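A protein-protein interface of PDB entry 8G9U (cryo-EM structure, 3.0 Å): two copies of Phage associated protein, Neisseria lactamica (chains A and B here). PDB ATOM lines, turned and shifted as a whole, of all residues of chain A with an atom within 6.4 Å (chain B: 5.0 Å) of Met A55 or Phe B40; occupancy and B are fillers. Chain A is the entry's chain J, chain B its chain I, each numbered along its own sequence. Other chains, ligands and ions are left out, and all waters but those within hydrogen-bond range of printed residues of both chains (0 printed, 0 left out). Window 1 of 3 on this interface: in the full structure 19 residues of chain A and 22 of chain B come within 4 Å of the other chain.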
ATOM      1  N   LEU A  16      12.259  33.837  12.895  1.00  0.00           N
ATOM      2  CA  LEU A  16      11.135  33.116  12.331  1.00  0.00           C
ATOM      3  C   LEU A  16       9.937  33.164  13.254  1.00  0.00           C
ATOM      4  O   LEU A  16       8.805  33.339  12.806  1.00  0.00           O
ATOM      5  CB  LEU A  16      11.554  31.681  12.083  1.00  0.00           C
ATOM      6  CG  LEU A  16      10.459  30.704  11.775  1.00  0.00           C
ATOM      7  CD1 LEU A  16       9.914  31.055  10.432  1.00  0.00           C
ATOM      8  CD2 LEU A  16      11.119  29.366  11.769  1.00  0.00           C
ATOM      9  N   LEU A  20       6.383  34.839  12.703  1.00  0.00           N
ATOM     10  CA  LEU A  20       5.213  33.995  12.899  1.00  0.00           C
ATOM     11  C   LEU A  20       4.201  34.681  13.800  1.00  0.00           C
ATOM     12  O   LEU A  20       3.005  34.723  13.491  1.00  0.00           O
ATOM     13  CB  LEU A  20       5.641  32.661  13.490  1.00  0.00           C
ATOM     14  CG  LEU A  20       6.200  31.632  12.524  1.00  0.00           C
ATOM     15  CD1 LEU A  20       6.617  30.412  13.284  1.00  0.00           C
ATOM     16  CD2 LEU A  20       5.155  31.284  11.526  1.00  0.00           C
ATOM     17  N   VAL A  50       7.243  22.958  18.605  1.00  0.00           N
ATOM     18  CA  VAL A  50       6.271  23.877  18.054  1.00  0.00           C
ATOM     19  C   VAL A  50       6.482  24.107  16.567  1.00  0.00           C
ATOM     20  O   VAL A  50       5.563  23.882  15.785  1.00  0.00           O
ATOM     21  CB  VAL A  50       6.285  25.201  18.833  1.00  0.00           C
ATOM     22  CG1 VAL A  50       5.738  24.974  20.199  1.00  0.00           C
ATOM     23  CG2 VAL A  50       7.680  25.669  18.961  1.00  0.00           C
ATOM     24  N   PHE A  51       7.678  24.518  16.146  1.00  0.00           N
ATOM     25  CA  PHE A  51       7.852  25.087  14.816  1.00  0.00           C
ATOM     26  C   PHE A  51       7.296  24.212  13.710  1.00  0.00           C
ATOM     27  O   PHE A  51       7.029  24.715  12.616  1.00  0.00           O
ATOM     28  CB  PHE A  51       9.321  25.381  14.573  1.00  0.00           C
ATOM     29  CG  PHE A  51       9.723  26.735  15.023  1.00  0.00           C
ATOM     30  CD1 PHE A  51       9.089  27.845  14.526  1.00  0.00           C
ATOM     31  CD2 PHE A  51      10.697  26.901  15.973  1.00  0.00           C
ATOM     32  CE1 PHE A  51       9.440  29.091  14.943  1.00  0.00           C
ATOM     33  CE2 PHE A  51      11.050  28.146  16.392  1.00  0.00           C
ATOM     34  CZ  PHE A  51      10.421  29.244  15.877  1.00  0.00           C
ATOM     35  N   GLY A  52       7.099  22.928  13.962  1.00  0.00           N
ATOM     36  CA  GLY A  52       6.268  22.164  13.066  1.00  0.00           C
ATOM     37  C   GLY A  52       4.846  22.681  13.111  1.00  0.00           C
ATOM     38  O   GLY A  52       4.278  23.043  12.079  1.00  0.00           O
ATOM     39  N   THR A  53       4.272  22.741  14.313  1.00  0.00           N
ATOM     40  CA  THR A  53       2.888  23.166  14.472  1.00  0.00           C
ATOM     41  C   THR A  53       2.701  24.633  14.156  1.00  0.00           C
ATOM     42  O   THR A  53       1.629  25.025  13.693  1.00  0.00           O
ATOM     43  CB  THR A  53       2.424  22.915  15.891  1.00  0.00           C
ATOM     44  OG1 THR A  53       2.971  23.927  16.736  1.00  0.00           O
ATOM     45  CG2 THR A  53       2.946  21.592  16.348  1.00  0.00           C
ATOM     46  N   LEU A  54       3.718  25.443  14.412  1.00  0.00           N
ATOM     47  CA  LEU A  54       3.691  26.854  14.072  1.00  0.00           C
ATOM     48  C   LEU A  54       3.495  27.069  12.591  1.00  0.00           C
ATOM     49  O   LEU A  54       3.100  28.161  12.170  1.00  0.00           O
ATOM     50  CB  LEU A  54       4.983  27.502  14.535  1.00  0.00           C
ATOM     51  CG  LEU A  54       4.874  27.913  15.981  1.00  0.00           C
ATOM     52  CD1 LEU A  54       6.157  28.491  16.465  1.00  0.00           C
ATOM     53  CD2 LEU A  54       3.833  28.980  15.942  1.00  0.00           C
ATOM     54  N   MET A  55       3.777  26.060  11.783  1.00  0.00           N
ATOM     55  CA  MET A  55       3.607  26.199  10.356  1.00  0.00           C
ATOM     56  C   MET A  55       2.549  25.283   9.772  1.00  0.00           C
ATOM     57  O   MET A  55       2.199  25.453   8.603  1.00  0.00           O
ATOM     58  CB  MET A  55       4.950  26.016   9.665  1.00  0.00           C
ATOM     59  CG  MET A  55       5.826  27.140  10.094  1.00  0.00           C
ATOM     60  SD  MET A  55       7.474  27.156   9.469  1.00  0.00           S
ATOM     61  CE  MET A  55       8.156  28.059  10.814  1.00  0.00           C
ATOM     62  N   ARG A  56       1.985  24.359  10.551  1.00  0.00           N
ATOM     63  CA  ARG A  56       0.592  24.026  10.292  1.00  0.00           C
ATOM     64  C   ARG A  56      -0.209  25.304  10.349  1.00  0.00           C
ATOM     65  O   ARG A  56      -1.049  25.580   9.488  1.00  0.00           O
ATOM     66  CB  ARG A  56       0.009  23.114  11.364  1.00  0.00           C
ATOM     67  CG  ARG A  56       0.216  21.638  11.361  1.00  0.00           C
ATOM     68  CD  ARG A  56       1.610  21.311  11.741  1.00  0.00           C
ATOM     69  NE  ARG A  56       1.707  19.903  12.067  1.00  0.00           N
ATOM     70  CZ  ARG A  56       2.834  19.293  12.384  1.00  0.00           C
ATOM     71  NH1 ARG A  56       3.970  19.964  12.397  1.00  0.00           N
ATOM     72  NH2 ARG A  56       2.817  18.014  12.712  1.00  0.00           N
ATOM     73  N   LEU A  57       0.079  26.098  11.371  1.00  0.00           N
ATOM     74  CA  LEU A  57      -0.696  27.215  11.869  1.00  0.00           C
ATOM     75  C   LEU A  57      -0.440  28.483  11.085  1.00  0.00           C
ATOM     76  O   LEU A  57      -1.207  29.442  11.198  1.00  0.00           O
ATOM     77  CB  LEU A  57      -0.319  27.406  13.338  1.00  0.00           C
ATOM     78  CG  LEU A  57      -0.977  28.362  14.298  1.00  0.00           C
ATOM     79  CD1 LEU A  57      -2.372  27.888  14.442  1.00  0.00           C
ATOM     80  CD2 LEU A  57      -0.264  28.326  15.630  1.00  0.00           C
ATOM     81  N   LEU A  58       0.626  28.498  10.299  1.00  0.00           N
ATOM     82  CA  LEU A  58       1.035  29.711   9.598  1.00  0.00           C
ATOM     83  C   LEU A  58       0.204  30.016   8.360  1.00  0.00           C
ATOM     84  O   LEU A  58      -0.248  31.166   8.222  1.00  0.00           O
ATOM     85  CB  LEU A  58       2.519  29.601   9.263  1.00  0.00           C
ATOM     86  CG  LEU A  58       3.089  30.630   8.316  1.00  0.00           C
ATOM     87  CD1 LEU A  58       2.908  32.001   8.885  1.00  0.00           C
ATOM     88  CD2 LEU A  58       4.538  30.297   8.159  1.00  0.00           C
ATOM     89  N   PRO A  59      -0.018  29.088   7.426  1.00  0.00           N
ATOM     90  CA  PRO A  59      -0.802  29.440   6.239  1.00  0.00           C
ATOM     91  C   PRO A  59      -2.179  29.933   6.581  1.00  0.00           C
ATOM     92  O   PRO A  59      -2.730  30.762   5.852  1.00  0.00           O
ATOM     93  CB  PRO A  59      -0.866  28.127   5.454  1.00  0.00           C
ATOM     94  CG  PRO A  59       0.250  27.329   5.957  1.00  0.00           C
ATOM     95  CD  PRO A  59       0.406  27.682   7.383  1.00  0.00           C
ATOM     96  N   HIS A  60      -2.750  29.466   7.681  1.00  0.00           N
ATOM     97  CA  HIS A  60      -4.052  29.949   8.094  1.00  0.00           C
ATOM     98  C   HIS A  60      -4.000  31.381   8.588  1.00  0.00           C
ATOM     99  O   HIS A  60      -4.949  32.134   8.356  1.00  0.00           O
ATOM    100  CB  HIS A  60      -4.602  29.031   9.164  1.00  0.00           C
ATOM    101  CG  HIS A  60      -4.312  27.594   8.899  1.00  0.00           C
ATOM    102  ND1 HIS A  60      -4.658  26.974   7.721  1.00  0.00           N
ATOM    103  CD2 HIS A  60      -3.688  26.661   9.649  1.00  0.00           C
ATOM    104  CE1 HIS A  60      -4.264  25.714   7.759  1.00  0.00           C
ATOM    105  NE2 HIS A  60      -3.673  25.499   8.919  1.00  0.00           N
ATOM    106  N   ILE A  78       9.458  35.068   6.013  1.00  0.00           N
ATOM    107  CA  ILE A  78       9.559  33.730   6.584  1.00  0.00           C
ATOM    108  C   ILE A  78      10.493  32.881   5.744  1.00  0.00           C
ATOM    109  O   ILE A  78      11.327  32.140   6.267  1.00  0.00           O
ATOM    110  CB  ILE A  78       8.184  33.065   6.698  1.00  0.00           C
ATOM    111  CG1 ILE A  78       7.311  33.809   7.672  1.00  0.00           C
ATOM    112  CG2 ILE A  78       8.330  31.644   7.168  1.00  0.00           C
ATOM    113  CD1 ILE A  78       5.943  33.357   7.566  1.00  0.00           C
ATOM    114  N   LEU A  82      13.977  31.221   6.704  1.00  0.00           N
ATOM    115  CA  LEU A  82      14.119  29.780   6.632  1.00  0.00           C
ATOM    116  C   LEU A  82      15.181  29.324   5.652  1.00  0.00           C
ATOM    117  O   LEU A  82      15.592  28.165   5.721  1.00  0.00           O
ATOM    118  CB  LEU A  82      12.779  29.136   6.290  1.00  0.00           C
ATOM    119  CG  LEU A  82      11.875  29.162   7.516  1.00  0.00           C
ATOM    120  CD1 LEU A  82      10.554  28.512   7.249  1.00  0.00           C
ATOM    121  CD2 LEU A  82      12.576  28.456   8.640  1.00  0.00           C
ATOM    122  N   PHE A  88      14.918  22.636  11.845  1.00  0.00           N
ATOM    123  CA  PHE A  88      14.565  23.091  13.173  1.00  0.00           C
ATOM    124  C   PHE A  88      15.343  22.233  14.150  1.00  0.00           C
ATOM    125  O   PHE A  88      15.131  21.016  14.182  1.00  0.00           O
ATOM    126  CB  PHE A  88      13.072  22.969  13.414  1.00  0.00           C
ATOM    127  CG  PHE A  88      12.265  23.911  12.598  1.00  0.00           C
ATOM    128  CD1 PHE A  88      12.757  25.142  12.277  1.00  0.00           C
ATOM    129  CD2 PHE A  88      11.026  23.558  12.131  1.00  0.00           C
ATOM    130  CE1 PHE A  88      12.028  26.012  11.519  1.00  0.00           C
ATOM    131  CE2 PHE A  88      10.293  24.422  11.365  1.00  0.00           C
ATOM    132  CZ  PHE A  88      10.795  25.652  11.061  1.00  0.00           C
ATOM    133  N   PHE B  17       5.469  20.029  -1.359  1.00  0.00           N
ATOM    134  CA  PHE B  17       4.269  20.791  -1.072  1.00  0.00           C
ATOM    135  C   PHE B  17       4.424  22.229  -1.515  1.00  0.00           C
ATOM    136  O   PHE B  17       3.459  22.861  -1.946  1.00  0.00           O
ATOM    137  CB  PHE B  17       3.959  20.728   0.411  1.00  0.00           C
ATOM    138  CG  PHE B  17       2.633  21.271   0.752  1.00  0.00           C
ATOM    139  CD1 PHE B  17       2.477  22.603   1.024  1.00  0.00           C
ATOM    140  CD2 PHE B  17       1.534  20.456   0.777  1.00  0.00           C
ATOM    141  CE1 PHE B  17       1.260  23.105   1.324  1.00  0.00           C
ATOM    142  CE2 PHE B  17       0.317  20.956   1.081  1.00  0.00           C
ATOM    143  CZ  PHE B  17       0.182  22.282   1.354  1.00  0.00           C
ATOM    144  N   ILE B  35      -3.567  25.048  -1.136  1.00  0.00           N
ATOM    145  CA  ILE B  35      -3.342  23.815  -0.398  1.00  0.00           C
ATOM    146  C   ILE B  35      -2.532  24.075   0.859  1.00  0.00           C
ATOM    147  O   ILE B  35      -2.543  23.261   1.778  1.00  0.00           O
ATOM    148  CB  ILE B  35      -2.681  22.753  -1.284  1.00  0.00           C
ATOM    149  CG1 ILE B  35      -1.360  23.273  -1.812  1.00  0.00           C
ATOM    150  CG2 ILE B  35      -3.603  22.340  -2.398  1.00  0.00           C
ATOM    151  CD1 ILE B  35      -0.568  22.231  -2.474  1.00  0.00           C
ATOM    152  N   ALA B  36      -1.831  25.200   0.946  1.00  0.00           N
ATOM    153  CA  ALA B  36      -1.305  25.580   2.250  1.00  0.00           C
ATOM    154  C   ALA B  36      -2.443  25.847   3.219  1.00  0.00           C
ATOM    155  O   ALA B  36      -2.394  25.455   4.389  1.00  0.00           O
ATOM    156  CB  ALA B  36      -0.410  26.806   2.136  1.00  0.00           C
ATOM    157  N   ARG B  38      -5.432  24.625   3.277  1.00  0.00           N
ATOM    158  CA  ARG B  38      -6.382  23.532   3.459  1.00  0.00           C
ATOM    159  C   ARG B  38      -5.721  22.179   3.705  1.00  0.00           C
ATOM    160  O   ARG B  38      -6.327  21.318   4.349  1.00  0.00           O
ATOM    161  CB  ARG B  38      -7.305  23.471   2.226  1.00  0.00           C
ATOM    162  CG  ARG B  38      -7.699  22.091   1.804  1.00  0.00           C
ATOM    163  CD  ARG B  38      -8.394  22.020   0.454  1.00  0.00           C
ATOM    164  NE  ARG B  38      -8.039  23.143  -0.413  1.00  0.00           N
ATOM    165  CZ  ARG B  38      -8.920  23.956  -0.988  1.00  0.00           C
ATOM    166  NH1 ARG B  38     -10.225  23.756  -0.826  1.00  0.00           N
ATOM    167  NH2 ARG B  38      -8.500  24.952  -1.754  1.00  0.00           N
ATOM    168  N   TYR B  39      -4.485  21.980   3.241  1.00  0.00           N
ATOM    169  CA  TYR B  39      -3.795  20.699   3.295  1.00  0.00           C
ATOM    170  C   TYR B  39      -2.528  20.728   4.133  1.00  0.00           C
ATOM    171  O   TYR B  39      -2.127  19.681   4.645  1.00  0.00           O
ATOM    172  CB  TYR B  39      -3.425  20.239   1.876  1.00  0.00           C
ATOM    173  CG  TYR B  39      -4.547  19.591   1.114  1.00  0.00           C
ATOM    174  CD1 TYR B  39      -5.770  19.410   1.681  1.00  0.00           C
ATOM    175  CD2 TYR B  39      -4.391  19.189  -0.188  1.00  0.00           C
ATOM    176  CE1 TYR B  39      -6.801  18.837   0.984  1.00  0.00           C
ATOM    177  CE2 TYR B  39      -5.423  18.608  -0.889  1.00  0.00           C
ATOM    178  CZ  TYR B  39      -6.628  18.437  -0.294  1.00  0.00           C
ATOM    179  OH  TYR B  39      -7.675  17.859  -0.982  1.00  0.00           O
ATOM    180  N   PHE B  40      -1.898  21.896   4.292  1.00  0.00           N
ATOM    181  CA  PHE B  40      -0.571  21.968   4.904  1.00  0.00           C
ATOM    182  C   PHE B  40      -0.557  21.341   6.288  1.00  0.00           C
ATOM    183  O   PHE B  40       0.421  20.695   6.672  1.00  0.00           O
ATOM    184  CB  PHE B  40      -0.105  23.422   4.989  1.00  0.00           C
ATOM    185  CG  PHE B  40       1.353  23.581   5.310  1.00  0.00           C
ATOM    186  CD1 PHE B  40       1.844  23.281   6.555  1.00  0.00           C
ATOM    187  CD2 PHE B  40       2.221  24.081   4.374  1.00  0.00           C
ATOM    188  CE1 PHE B  40       3.167  23.427   6.839  1.00  0.00           C
ATOM    189  CE2 PHE B  40       3.547  24.237   4.666  1.00  0.00           C
ATOM    190  CZ  PHE B  40       4.018  23.911   5.901  1.00  0.00           C
ATOM    191  N   GLY B  41      -1.630  21.515   7.050  1.00  0.00           N
ATOM    192  CA  GLY B  41      -1.626  21.038   8.419  1.00  0.00           C
ATOM    193  C   GLY B  41      -1.293  19.563   8.528  1.00  0.00           C
ATOM    194  O   GLY B  41      -0.601  19.142   9.454  1.00  0.00           O
ATOM    195  N   SER B  42      -1.771  18.764   7.582  1.00  0.00           N
ATOM    196  CA  SER B  42      -1.455  17.345   7.605  1.00  0.00           C
ATOM    197  C   SER B  42      -0.329  16.996   6.654  1.00  0.00           C
ATOM    198  O   SER B  42       0.438  16.073   6.926  1.00  0.00           O
ATOM    199  CB  SER B  42      -2.679  16.525   7.245  1.00  0.00           C
ATOM    200  OG  SER B  42      -3.126  16.934   5.978  1.00  0.00           O
ATOM    201  N   ALA B  43      -0.202  17.718   5.543  1.00  0.00           N
ATOM    202  CA  ALA B  43       0.945  17.508   4.676  1.00  0.00           C
ATOM    203  C   ALA B  43       2.231  17.615   5.460  1.00  0.00           C
ATOM    204  O   ALA B  43       3.176  16.864   5.215  1.00  0.00           O
ATOM    205  CB  ALA B  43       0.938  18.520   3.539  1.00  0.00           C
ATOM    206  N   SER B  44       2.269  18.513   6.434  1.00  0.00           N
ATOM    207  CA  SER B  44       3.403  18.618   7.325  1.00  0.00           C
ATOM    208  C   SER B  44       3.454  17.494   8.337  1.00  0.00           C
ATOM    209  O   SER B  44       4.534  17.184   8.836  1.00  0.00           O
ATOM    210  CB  SER B  44       3.360  19.954   8.055  1.00  0.00           C
ATOM    211  OG  SER B  44       4.436  20.070   8.961  1.00  0.00           O
ATOM    212  N   SER B  45       2.335  16.871   8.645  1.00  0.00           N
ATOM    213  CA  SER B  45       2.332  15.850   9.679  1.00  0.00           C
ATOM    214  C   SER B  45       1.935  14.475   9.178  1.00  0.00           C
ATOM    215  O   SER B  45       2.529  13.484   9.593  1.00  0.00           O
ATOM    216  CB  SER B  45       1.404  16.262  10.823  1.00  0.00           C
ATOM    217  OG  SER B  45       0.063  16.365  10.395  1.00  0.00           O
ATOM    218  N   PHE B 100       9.599  19.704   7.141  1.00  0.00           N
ATOM    219  CA  PHE B 100       8.587  19.939   6.122  1.00  0.00           C
ATOM    220  C   PHE B 100       8.321  21.423   5.957  1.00  0.00           C
ATOM    221  O   PHE B 100       8.192  21.918   4.840  1.00  0.00           O
ATOM    222  CB  PHE B 100       7.295  19.213   6.459  1.00  0.00           C
ATOM    223  CG  PHE B 100       6.235  19.377   5.419  1.00  0.00           C
ATOM    224  CD1 PHE B 100       5.482  20.530   5.352  1.00  0.00           C
ATOM    225  CD2 PHE B 100       5.991  18.381   4.511  1.00  0.00           C
ATOM    226  CE1 PHE B 100       4.522  20.681   4.408  1.00  0.00           C
ATOM    227  CE2 PHE B 100       5.026  18.533   3.563  1.00  0.00           C
ATOM    228  CZ  PHE B 100       4.288  19.681   3.519  1.00  0.00           C
ATOM    229  N   ALA B 101       8.172  22.143   7.061  1.00  0.00           N
ATOM    230  CA  ALA B 101       7.999  23.583   6.959  1.00  0.00           C
ATOM    231  C   ALA B 101       9.241  24.223   6.370  1.00  0.00           C
ATOM    232  O   ALA B 101       9.154  25.150   5.552  1.00  0.00           O
ATOM    233  CB  ALA B 101       7.689  24.155   8.332  1.00  0.00           C
ATOM    234  N   TYR B 104       8.891  23.542   2.649  1.00  0.00           N
ATOM    235  CA  TYR B 104       7.903  24.430   2.076  1.00  0.00           C
ATOM    236  C   TYR B 104       8.505  25.793   1.819  1.00  0.00           C
ATOM    237  O   TYR B 104       8.423  26.312   0.707  1.00  0.00           O
ATOM    238  CB  TYR B 104       6.698  24.531   2.995  1.00  0.00           C
ATOM    239  CG  TYR B 104       5.651  25.425   2.433  1.00  0.00           C
ATOM    240  CD1 TYR B 104       4.849  25.019   1.398  1.00  0.00           C
ATOM    241  CD2 TYR B 104       5.476  26.687   2.935  1.00  0.00           C
ATOM    242  CE1 TYR B 104       3.902  25.849   0.885  1.00  0.00           C
ATOM    243  CE2 TYR B 104       4.538  27.515   2.432  1.00  0.00           C
ATOM    244  CZ  TYR B 104       3.756  27.101   1.412  1.00  0.00           C
ATOM    245  OH  TYR B 104       2.813  27.966   0.926  1.00  0.00           O
ATOM    246  N   TYR B 105       9.179  26.360   2.802  1.00  0.00           N
ATOM    247  CA  TYR B 105       9.626  27.724   2.592  1.00  0.00           C
ATOM    248  C   TYR B 105      10.937  27.821   1.828  1.00  0.00           C
ATOM    249  O   TYR B 105      11.122  28.778   1.077  1.00  0.00           O
ATOM    250  CB  TYR B 105       9.683  28.439   3.929  1.00  0.00           C
ATOM    251  CG  TYR B 105       8.286  28.807   4.325  1.00  0.00           C
ATOM    252  CD1 TYR B 105       7.525  29.602   3.506  1.00  0.00           C
ATOM    253  CD2 TYR B 105       7.692  28.274   5.441  1.00  0.00           C
ATOM    254  CE1 TYR B 105       6.254  29.928   3.818  1.00  0.00           C
ATOM    255  CE2 TYR B 105       6.401  28.586   5.763  1.00  0.00           C
ATOM    256  CZ  TYR B 105       5.686  29.418   4.941  1.00  0.00           C
ATOM    257  OH  TYR B 105       4.386  29.750   5.225  1.00  0.00           O
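The side-chain hydroxyl of Ser B44 sits at hydrogen-bond distance from the guanidinium group of Arg A56, 3.5 Å away.
The backbone NH (N) of Phe B40 lies within hydrogen-bond range of the backbone carbonyl oxygen (O) of Ile B35 (2.9 Å). The side-chain hydroxyl of Ser B45 is in hydrogen-bond range of the backbone carbonyl oxygen of Gly B41 (3.0 Å). The guanidinium group (NH1) of Arg A56 lies close to the backbone carbonyl oxygen (O) of Gly A52 (3.1 Å). A ring nitrogen (NE2) of His A60 is in hydrogen-bond range of the backbone carbonyl oxygen of Arg A56 (2.7 Å).
Among the printed residues, merely in contact across the chains: Met A55 with Phe B40 (2.9 Å), Arg A56 with Ser B45 (2.9 Å), Leu A58 with Tyr B105 (3.0 Å), Met A55 with Ala B101 (3.2 Å), Arg A56 with Gly B41 (3.2 Å), Pro A59 with Ala B36 (3.3 Å), Leu A82 with Tyr B105 (3.4 Å), Ile A78 with Tyr B105 (3.8 Å), His A60 with Ala B36 (3.9 Å) and Pro A59 with Phe B40 (3.96 Å).
Gly A52 touches none of the printed residues of chain B. Met A55 touches just these residues of chain B: Phe B40 and Ala B101. Of the printed residues of chain B, Arg A56 touches Gly B41, Ser B44 and Ser B45. Of the printed residues of chain B, His A60 touches Ala B36. Printed residues of chain B within 4 Å of Leu A82: Tyr B105. Printed residues of chain A within 4 Å of Phe B40: Met A55 and Pro A59. Ser B42 touches none of the printed residues of chain A. Of the printed residues of chain A, Ser B44 touches Arg A56. Printed residues of chain A within 4 Å of Tyr B105: Leu A58, Ile A78 and Leu A82. The nearest residue of chain B that does not touch Met A55 is Tyr B105 (4.1 Å).
Printed residues of chain A that touch a printed residue of chain B: Met A55, Arg A56, Leu A58, Pro A59, His A60, Ile A78 and Leu A82. Hydrophobic or aromatic side chains of chain B that line the printed part of chain A: Ala B36, Phe B40, Ala B101 and Tyr B105. Among the printed residues, 11 pairs touch across the chains. Among the printed residues, no Asp or Glu carboxylate lies within 4 Å of a Lys or Arg side-chain nitrogen of the other chain.
No position is printed for both chains. Of the 11 pairs that touch across the chains among the printed residues, none has its exchanged pair printed and touching as well.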
